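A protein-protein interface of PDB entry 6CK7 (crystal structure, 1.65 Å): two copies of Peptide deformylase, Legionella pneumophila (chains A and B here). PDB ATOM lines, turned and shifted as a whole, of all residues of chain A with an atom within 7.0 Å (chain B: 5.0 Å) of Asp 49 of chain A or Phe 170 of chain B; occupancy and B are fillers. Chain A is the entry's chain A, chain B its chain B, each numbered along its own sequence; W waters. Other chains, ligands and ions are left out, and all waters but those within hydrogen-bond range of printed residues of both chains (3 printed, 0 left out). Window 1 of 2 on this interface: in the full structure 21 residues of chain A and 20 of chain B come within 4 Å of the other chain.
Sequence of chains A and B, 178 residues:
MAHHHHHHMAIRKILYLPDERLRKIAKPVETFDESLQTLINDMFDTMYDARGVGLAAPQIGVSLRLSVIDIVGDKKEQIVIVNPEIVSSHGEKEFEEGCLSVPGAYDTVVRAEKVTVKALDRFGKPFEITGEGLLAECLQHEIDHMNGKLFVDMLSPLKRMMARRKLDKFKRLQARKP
NZ of Lys 177 of chain B lies within salt-bridge range of OD2 of Asp 49 of chain A (3.6 Å).
The side-chain carboxylate of Asp 49 of chain A sits close to the side-chain amide nitrogen of Gln 174 of chain B, at 3.3 Å.
Printed residues of chain B that touch a printed residue of chain A: Pro 103, Lys 169, Phe 170, Leu 173, Gln 174 and Lys 177.
Hydrophobic or aromatic side chains of chain B that line the printed part of chain A: Pro 103, Phe 170 and Leu 173.
Along chain B the printed residues that touch a printed residue of chain A span positions 103 to 177.
Of the 13 printed residues of chain A, 5 touch a printed residue of chain B.
Among the printed residues, 10 pairs touch across the chains.
Leu 173 of chain B touches Ile 11 of chain A (O to CD1, 3.5 Å).
Asp 45 of chain A touches Leu 173 of chain B (OD1 to CD2, 3.7 Å).
CE of Lys 169 of chain B touches CD2 of Tyr 48 of chain A, at 3.8 Å.
CD1 of Phe 170 of chain B touches O of Tyr 48 of chain A (3.7 Å).
Tyr 48 of chain A touches Leu 173 of chain B.
Asp 49 of chain A touches Phe 170 of chain B (O to CE1, 3.4 Å).
Asp 49 of chain A touches Leu 173 of chain B (OD1 to C, 3.7 Å).
Arg 51 of chain A touches Pro 103 of chain B (CZ to CA, 3.6 Å).
Of chain B, only Phe 170 (3.4 Å), Leu 173 (3.7 Å), Gln 174 (2.4 Å) and Lys 177 (3.3 Å) come within 4 Å of Asp 49 of chain A.
Of the printed residues of chain A, Pro 103 of chain B touches Arg 51.
Printed residues of chain A within 4 Å of Phe 170 of chain B: Tyr 48 and Asp 49.
Of the printed residues of chain A, Leu 173 of chain B touches Ile 11, Asp 45, Tyr 48 and Asp 49.
Of the printed residues of chain A, Lys 177 of chain B touches Asp 49.
The nearest printed residue of chain B that does not touch Asp 49 of chain A is Arg 172 of chain B (6.5 Å).
The nearest printed residue of chain A that does not touch Phe 170 of chain B is Arg 51 of chain A (4.03 Å).
The nearest printed residue of chain A that does not touch Lys 169 of chain B is Asp 45 of chain A (4.7 Å).
Water W2 lies within hydrogen-bond range of the side-chain carboxylate of Asp 45 of chain A (2.7 Å) and the side-chain amino group of Lys 169 of chain B (2.9 Å).
Water W3 bridges NZ of Lys 166 of chain B and O of Gly 52 of chain A.
Water W1 bridges O of Gly 52 of chain A (2.8 Å) and NZ of Lys 166 of chain B (3.0 Å).
No position is printed for both chains.
Of the 10 pairs that touch across the chains among the printed residues, none has its exchanged pair printed and touching as well.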
ATOM      1  N   ILE A  11       7.111   3.525  -8.644  1.00  0.00           N
ATOM      2  CA  ILE A  11       6.860   2.109  -8.420  1.00  0.00           C
ATOM      3  C   ILE A  11       6.211   1.933  -7.049  1.00  0.00           C
ATOM      4  O   ILE A  11       6.623   2.555  -6.060  1.00  0.00           O
ATOM      5  CB  ILE A  11       8.186   1.339  -8.536  1.00  0.00           C
ATOM      6  CG1 ILE A  11       8.646   1.325 -10.005  1.00  0.00           C
ATOM      7  CG2 ILE A  11       8.044  -0.060  -7.959  1.00  0.00           C
ATOM      8  CD1 ILE A  11      10.113   0.955 -10.191  1.00  0.00           C
ATOM      9  N   ARG A  12       5.178   1.096  -6.985  1.00  0.00           N
ATOM     10  CA  ARG A  12       4.350   0.990  -5.792  1.00  0.00           C
ATOM     11  C   ARG A  12       4.693  -0.258  -4.989  1.00  0.00           C
ATOM     12  O   ARG A  12       5.171  -1.262  -5.529  1.00  0.00           O
ATOM     13  CB  ARG A  12       2.863   0.965  -6.160  1.00  0.00           C
ATOM     14  CG  ARG A  12       2.462   2.036  -7.149  1.00  0.00           C
ATOM     15  CD  ARG A  12       2.626   3.447  -6.598  1.00  0.00           C
ATOM     16  NE  ARG A  12       2.172   4.401  -7.599  1.00  0.00           N
ATOM     17  CZ  ARG A  12       0.908   4.801  -7.711  1.00  0.00           C
ATOM     18  NH1 ARG A  12       0.004   4.354  -6.852  1.00  0.00           N
ATOM     19  NH2 ARG A  12       0.548   5.639  -8.673  1.00  0.00           N
ATOM     20  N   ILE A  14       3.842  -3.611  -3.320  1.00  0.00           N
ATOM     21  CA  ILE A  14       2.887  -4.703  -3.499  1.00  0.00           C
ATOM     22  C   ILE A  14       2.574  -5.289  -2.127  1.00  0.00           C
ATOM     23  O   ILE A  14       3.484  -5.581  -1.334  1.00  0.00           O
ATOM     24  CB  ILE A  14       3.456  -5.768  -4.445  1.00  0.00           C
ATOM     25  CG1 ILE A  14       3.663  -5.167  -5.839  1.00  0.00           C
ATOM     26  CG2 ILE A  14       2.553  -7.000  -4.501  1.00  0.00           C
ATOM     27  CD1 ILE A  14       4.390  -6.076  -6.791  1.00  0.00           C
ATOM     28  N   MET A  43       1.418   0.954 -12.375  1.00  0.00           N
ATOM     29  CA  MET A  43       1.127  -0.469 -12.228  1.00  0.00           C
ATOM     30  C   MET A  43       1.960  -1.311 -13.186  1.00  0.00           C
ATOM     31  O   MET A  43       2.495  -2.351 -12.786  1.00  0.00           O
ATOM     32  CB  MET A  43      -0.367  -0.718 -12.431  1.00  0.00           C
ATOM     33  CG  MET A  43      -1.162  -0.277 -11.199  1.00  0.00           C
ATOM     34  SD  MET A  43      -2.941  -0.543 -11.423  1.00  0.00           S
ATOM     35  CE  MET A  43      -3.003  -2.329 -11.610  1.00  0.00           C
ATOM     36  N   PHE A  44       2.076  -0.897 -14.454  1.00  0.00           N
ATOM     37  CA  PHE A  44       2.949  -1.637 -15.368  1.00  0.00           C
ATOM     38  C   PHE A  44       4.384  -1.652 -14.848  1.00  0.00           C
ATOM     39  O   PHE A  44       5.028  -2.705 -14.796  1.00  0.00           O
ATOM     40  CB  PHE A  44       2.900  -1.037 -16.775  1.00  0.00           C
ATOM     41  CG  PHE A  44       1.765  -1.548 -17.623  1.00  0.00           C
ATOM     42  CD1 PHE A  44       1.712  -2.856 -18.025  1.00  0.00           C
ATOM     43  CD2 PHE A  44       0.751  -0.704 -18.031  1.00  0.00           C
ATOM     44  CE1 PHE A  44       0.650  -3.302 -18.828  1.00  0.00           C
ATOM     45  CE2 PHE A  44      -0.300  -1.167 -18.828  1.00  0.00           C
ATOM     46  CZ  PHE A  44      -0.351  -2.458 -19.207  1.00  0.00           C
ATOM     47  N   ASP A  45       4.900  -0.485 -14.452  1.00  0.00           N
ATOM     48  CA  ASP A  45       6.251  -0.420 -13.903  1.00  0.00           C
ATOM     49  C   ASP A  45       6.405  -1.358 -12.716  1.00  0.00           C
ATOM     50  O   ASP A  45       7.407  -2.077 -12.597  1.00  0.00           O
ATOM     51  CB  ASP A  45       6.573   1.015 -13.476  1.00  0.00           C
ATOM     52  CG  ASP A  45       6.803   1.951 -14.650  1.00  0.00           C
ATOM     53  OD1 ASP A  45       6.860   1.505 -15.812  1.00  0.00           O
ATOM     54  OD2 ASP A  45       6.950   3.160 -14.393  1.00  0.00           O
ATOM     55  N   THR A  46       5.412  -1.368 -11.831  1.00  0.00           N
ATOM     56  CA  THR A  46       5.464  -2.192 -10.628  1.00  0.00           C
ATOM     57  C   THR A  46       5.441  -3.673 -10.986  1.00  0.00           C
ATOM     58  O   THR A  46       6.218  -4.471 -10.441  1.00  0.00           O
ATOM     59  CB  THR A  46       4.289  -1.809  -9.713  1.00  0.00           C
ATOM     60  OG1 THR A  46       4.433  -0.432  -9.338  1.00  0.00           O
ATOM     61  CG2 THR A  46       4.287  -2.658  -8.462  1.00  0.00           C
ATOM     62  N   MET A  47       4.566  -4.040 -11.924  1.00  0.00           N
ATOM     63  CA  MET A  47       4.477  -5.418 -12.392  1.00  0.00           C
ATOM     64  C   MET A  47       5.800  -5.899 -12.971  1.00  0.00           C
ATOM     65  O   MET A  47       6.305  -6.965 -12.595  1.00  0.00           O
ATOM     66  CB  MET A  47       3.365  -5.527 -13.442  1.00  0.00           C
ATOM     67  CG  MET A  47       3.175  -6.918 -13.986  1.00  0.00           C
ATOM     68  SD  MET A  47       2.196  -6.875 -15.522  1.00  0.00           S
ATOM     69  CE  MET A  47       3.458  -6.366 -16.653  1.00  0.00           C
ATOM     70  N   TYR A  48       6.376  -5.133 -13.903  1.00  0.00           N
ATOM     71  CA  TYR A  48       7.643  -5.567 -14.494  1.00  0.00           C
ATOM     72  C   TYR A  48       8.744  -5.611 -13.446  1.00  0.00           C
ATOM     73  O   TYR A  48       9.577  -6.532 -13.442  1.00  0.00           O
ATOM     74  CB  TYR A  48       8.060  -4.642 -15.639  1.00  0.00           C
ATOM     75  CG  TYR A  48       7.157  -4.647 -16.858  1.00  0.00           C
ATOM     76  CD1 TYR A  48       6.919  -5.813 -17.582  1.00  0.00           C
ATOM     77  CD2 TYR A  48       6.570  -3.467 -17.303  1.00  0.00           C
ATOM     78  CE1 TYR A  48       6.103  -5.798 -18.719  1.00  0.00           C
ATOM     79  CE2 TYR A  48       5.763  -3.440 -18.415  1.00  0.00           C
ATOM     80  CZ  TYR A  48       5.519  -4.610 -19.118  1.00  0.00           C
ATOM     81  OH  TYR A  48       4.713  -4.587 -20.226  1.00  0.00           O
ATOM     82  N   ASP A  49       8.792  -4.608 -12.568  1.00  0.00           N
ATOM     83  CA  ASP A  49       9.839  -4.579 -11.559  1.00  0.00           C
ATOM     84  C   ASP A  49       9.734  -5.763 -10.610  1.00  0.00           C
ATOM     85  O   ASP A  49      10.747  -6.178 -10.028  1.00  0.00           O
ATOM     86  CB  ASP A  49       9.784  -3.269 -10.782  1.00  0.00           C
ATOM     87  CG  ASP A  49      10.890  -3.162  -9.796  1.00  0.00           C
ATOM     88  OD1 ASP A  49      12.040  -3.027 -10.253  1.00  0.00           O
ATOM     89  OD2 ASP A  49      10.617  -3.251  -8.586  1.00  0.00           O
ATOM     90  N   ALA A  50       8.533  -6.322 -10.449  1.00  0.00           N
ATOM     91  CA  ALA A  50       8.310  -7.468  -9.585  1.00  0.00           C
ATOM     92  C   ALA A  50       8.349  -8.791 -10.346  1.00  0.00           C
ATOM     93  O   ALA A  50       8.051  -9.834  -9.753  1.00  0.00           O
ATOM     94  CB  ALA A  50       6.958  -7.319  -8.869  1.00  0.00           C
ATOM     95  N   ARG A  51       8.712  -8.766 -11.640  1.00  0.00           N
ATOM     96  CA  ARG A  51       8.837  -9.973 -12.474  1.00  0.00           C
ATOM     97  C   ARG A  51       7.502 -10.697 -12.655  1.00  0.00           C
ATOM     98  O   ARG A  51       7.467 -11.926 -12.767  1.00  0.00           O
ATOM     99  CB  ARG A  51       9.896 -10.924 -11.916  1.00  0.00           C
ATOM    100  CG  ARG A  51      11.196 -10.214 -11.511  1.00  0.00           C
ATOM    101  CD  ARG A  51      12.034 -11.066 -10.577  1.00  0.00           C
ATOM    102  NE  ARG A  51      12.432 -12.320 -11.206  1.00  0.00           N
ATOM    103  CZ  ARG A  51      13.540 -12.992 -10.912  1.00  0.00           C
ATOM    104  NH1 ARG A  51      13.810 -14.126 -11.548  1.00  0.00           N
ATOM    105  NH2 ARG A  51      14.377 -12.529  -9.989  1.00  0.00           N
ATOM    106  N   GLY A  52       6.403  -9.941 -12.697  1.00  0.00           N
ATOM    107  CA  GLY A  52       5.092 -10.512 -12.931  1.00  0.00           C
ATOM    108  C   GLY A  52       4.636 -10.327 -14.370  1.00  0.00           C
ATOM    109  O   GLY A  52       5.253  -9.612 -15.157  1.00  0.00           O
ATOM    110  N   TYR B  16      22.863 -11.299 -12.590  1.00  0.00           N
ATOM    111  CA  TYR B  16      22.018 -11.366 -13.775  1.00  0.00           C
ATOM    112  C   TYR B  16      22.876 -11.409 -15.031  1.00  0.00           C
ATOM    113  O   TYR B  16      23.996 -10.894 -15.050  1.00  0.00           O
ATOM    114  CB  TYR B  16      21.080 -10.154 -13.868  1.00  0.00           C
ATOM    115  CG  TYR B  16      20.305  -9.834 -12.601  1.00  0.00           C
ATOM    116  CD1 TYR B  16      19.831 -10.839 -11.766  1.00  0.00           C
ATOM    117  CD2 TYR B  16      20.038  -8.516 -12.257  1.00  0.00           C
ATOM    118  CE1 TYR B  16      19.118 -10.529 -10.603  1.00  0.00           C
ATOM    119  CE2 TYR B  16      19.327  -8.198 -11.117  1.00  0.00           C
ATOM    120  CZ  TYR B  16      18.874  -9.198 -10.290  1.00  0.00           C
ATOM    121  OH  TYR B  16      18.168  -8.843  -9.150  1.00  0.00           O
ATOM    122  N   PRO B 103      15.917 -12.124 -14.562  1.00  0.00           N
ATOM    123  CA  PRO B 103      14.652 -11.620 -14.007  1.00  0.00           C
ATOM    124  C   PRO B 103      13.705 -11.124 -15.083  1.00  0.00           C
ATOM    125  O   PRO B 103      14.094 -10.379 -15.983  1.00  0.00           O
ATOM    126  CB  PRO B 103      15.100 -10.471 -13.089  1.00  0.00           C
ATOM    127  CG  PRO B 103      16.570 -10.289 -13.322  1.00  0.00           C
ATOM    128  CD  PRO B 103      17.096 -11.538 -13.911  1.00  0.00           C
ATOM    129  N   LYS B 166      13.485  -7.465 -22.296  1.00  0.00           N
ATOM    130  CA  LYS B 166      12.720  -7.511 -21.052  1.00  0.00           C
ATOM    131  C   LYS B 166      13.639  -7.384 -19.843  1.00  0.00           C
ATOM    132  O   LYS B 166      13.307  -6.710 -18.859  1.00  0.00           O
ATOM    133  CB  LYS B 166      11.928  -8.809 -20.982  1.00  0.00           C
ATOM    134  CG  LYS B 166      11.012  -8.868 -19.797  1.00  0.00           C
ATOM    135  CD  LYS B 166       9.873  -9.832 -20.003  1.00  0.00           C
ATOM    136  CE  LYS B 166       8.756  -9.459 -19.058  1.00  0.00           C
ATOM    137  NZ  LYS B 166       7.890 -10.622 -18.697  1.00  0.00           N
ATOM    138  N   LEU B 167      14.795  -8.038 -19.899  1.00  0.00           N
ATOM    139  CA  LEU B 167      15.769  -7.927 -18.820  1.00  0.00           C
ATOM    140  C   LEU B 167      16.346  -6.520 -18.737  1.00  0.00           C
ATOM    141  O   LEU B 167      16.591  -6.009 -17.636  1.00  0.00           O
ATOM    142  CB  LEU B 167      16.883  -8.958 -19.024  1.00  0.00           C
ATOM    143  CG  LEU B 167      18.077  -8.903 -18.070  1.00  0.00           C
ATOM    144  CD1 LEU B 167      17.634  -9.050 -16.617  1.00  0.00           C
ATOM    145  CD2 LEU B 167      19.071  -9.981 -18.457  1.00  0.00           C
ATOM    146  N   ASP B 168      16.597  -5.883 -19.886  1.00  0.00           N
ATOM    147  CA  ASP B 168      17.095  -4.511 -19.859  1.00  0.00           C
ATOM    148  C   ASP B 168      16.065  -3.565 -19.253  1.00  0.00           C
ATOM    149  O   ASP B 168      16.427  -2.637 -18.522  1.00  0.00           O
ATOM    150  CB  ASP B 168      17.473  -4.045 -21.262  1.00  0.00           C
ATOM    151  CG  ASP B 168      18.720  -4.722 -21.777  1.00  0.00           C
ATOM    152  OD1 ASP B 168      19.409  -5.387 -20.974  1.00  0.00           O
ATOM    153  OD2 ASP B 168      19.005  -4.588 -22.983  1.00  0.00           O
ATOM    154  N   LYS B 169      14.784  -3.767 -19.568  1.00  0.00           N
ATOM    155  CA  LYS B 169      13.743  -2.921 -18.982  1.00  0.00           C
ATOM    156  C   LYS B 169      13.663  -3.128 -17.474  1.00  0.00           C
ATOM    157  O   LYS B 169      13.474  -2.168 -16.716  1.00  0.00           O
ATOM    158  CB  LYS B 169      12.395  -3.206 -19.642  1.00  0.00           C
ATOM    159  CG  LYS B 169      11.188  -2.724 -18.835  1.00  0.00           C
ATOM    160  CD  LYS B 169      10.110  -2.119 -19.724  1.00  0.00           C
ATOM    161  CE  LYS B 169       9.165  -1.207 -18.938  1.00  0.00           C
ATOM    162  NZ  LYS B 169       8.246  -0.512 -19.863  1.00  0.00           N
ATOM    163  N   PHE B 170      13.787  -4.378 -17.023  1.00  0.00           N
ATOM    164  CA  PHE B 170      13.800  -4.666 -15.592  1.00  0.00           C
ATOM    165  C   PHE B 170      14.922  -3.913 -14.897  1.00  0.00           C
ATOM    166  O   PHE B 170      14.729  -3.325 -13.823  1.00  0.00           O
ATOM    167  CB  PHE B 170      13.965  -6.170 -15.359  1.00  0.00           C
ATOM    168  CG  PHE B 170      14.288  -6.529 -13.934  1.00  0.00           C
ATOM    169  CD1 PHE B 170      13.276  -6.633 -12.987  1.00  0.00           C
ATOM    170  CD2 PHE B 170      15.600  -6.761 -13.541  1.00  0.00           C
ATOM    171  CE1 PHE B 170      13.565  -6.957 -11.678  1.00  0.00           C
ATOM    172  CE2 PHE B 170      15.900  -7.085 -12.236  1.00  0.00           C
ATOM    173  CZ  PHE B 170      14.879  -7.190 -11.301  1.00  0.00           C
ATOM    174  N   LYS B 171      16.113  -3.929 -15.498  1.00  0.00           N
ATOM    175  CA  LYS B 171      17.246  -3.225 -14.909  1.00  0.00           C
ATOM    176  C   LYS B 171      16.991  -1.729 -14.825  1.00  0.00           C
ATOM    177  O   LYS B 171      17.388  -1.087 -13.848  1.00  0.00           O
ATOM    178  CB  LYS B 171      18.511  -3.507 -15.716  1.00  0.00           C
ATOM    179  CG  LYS B 171      18.954  -4.947 -15.617  1.00  0.00           C
ATOM    180  CD  LYS B 171      20.210  -5.159 -16.420  1.00  0.00           C
ATOM    181  CE  LYS B 171      20.705  -6.590 -16.293  1.00  0.00           C
ATOM    182  NZ  LYS B 171      21.979  -6.786 -17.038  1.00  0.00           N
ATOM    183  N   ARG B 172      16.322  -1.154 -15.835  1.00  0.00           N
ATOM    184  CA  ARG B 172      16.027   0.277 -15.794  1.00  0.00           C
ATOM    185  C   ARG B 172      15.036   0.599 -14.681  1.00  0.00           C
ATOM    186  O   ARG B 172      15.186   1.604 -13.974  1.00  0.00           O
ATOM    187  CB  ARG B 172      15.482   0.753 -17.144  1.00  0.00           C
ATOM    188  CG  ARG B 172      16.481   0.669 -18.293  1.00  0.00           C
ATOM    189  CD  ARG B 172      15.959   1.370 -19.544  1.00  0.00           C
ATOM    190  NE  ARG B 172      14.652   0.867 -19.972  1.00  0.00           N
ATOM    191  CZ  ARG B 172      14.467  -0.026 -20.941  1.00  0.00           C
ATOM    192  NH1 ARG B 172      15.505  -0.537 -21.593  1.00  0.00           N
ATOM    193  NH2 ARG B 172      13.239  -0.415 -21.256  1.00  0.00           N
ATOM    194  N   LEU B 173      14.026  -0.254 -14.505  1.00  0.00           N
ATOM    195  CA  LEU B 173      13.060  -0.052 -13.432  1.00  0.00           C
ATOM    196  C   LEU B 173      13.711  -0.204 -12.065  1.00  0.00           C
ATOM    197  O   LEU B 173      13.421   0.571 -11.146  1.00  0.00           O
ATOM    198  CB  LEU B 173      11.903  -1.038 -13.588  1.00  0.00           C
ATOM    199  CG  LEU B 173      11.056  -0.746 -14.818  1.00  0.00           C
ATOM    200  CD1 LEU B 173      10.177  -1.947 -15.130  1.00  0.00           C
ATOM    201  CD2 LEU B 173      10.220   0.531 -14.633  1.00  0.00           C
ATOM    202  N   GLN B 174      14.593  -1.192 -11.911  1.00  0.00           N
ATOM    203  CA  GLN B 174      15.280  -1.373 -10.637  1.00  0.00           C
ATOM    204  C   GLN B 174      16.029  -0.114 -10.242  1.00  0.00           C
ATOM    205  O   GLN B 174      16.068   0.249  -9.060  1.00  0.00           O
ATOM    206  CB  GLN B 174      16.238  -2.562 -10.712  1.00  0.00           C
ATOM    207  CG  GLN B 174      15.532  -3.904 -10.667  1.00  0.00           C
ATOM    208  CD  GLN B 174      15.081  -4.263  -9.268  1.00  0.00           C
ATOM    209  OE1 GLN B 174      15.861  -4.775  -8.458  1.00  0.00           O
ATOM    210  NE2 GLN B 174      13.822  -3.974  -8.963  1.00  0.00           N
ATOM    211  N   LYS B 177      13.588   2.287  -8.661  1.00  0.00           N
ATOM    212  CA  LYS B 177      12.929   1.883  -7.432  1.00  0.00           C
ATOM    213  C   LYS B 177      13.496   2.701  -6.275  1.00  0.00           C
ATOM    214  O   LYS B 177      14.691   3.005  -6.265  1.00  0.00           O
ATOM    215  CB  LYS B 177      13.143   0.388  -7.193  1.00  0.00           C
ATOM    216  CG  LYS B 177      12.154  -0.276  -6.256  1.00  0.00           C
ATOM    217  CD  LYS B 177      12.406  -1.770  -6.250  1.00  0.00           C
ATOM    218  CE  LYS B 177      11.756  -2.448  -5.067  1.00  0.00           C
ATOM    219  NZ  LYS B 177      11.711  -3.923  -5.258  1.00  0.00           N
HETATM  220  O   HOH W   1       8.006  -9.952 -15.785  1.00  0.00           O
HETATM  221  O   HOH W   2       6.195  -0.101 -17.926  1.00  0.00           O
HETATM  222  O   HOH W   3       5.591  -9.204 -18.045  1.00  0.00           O
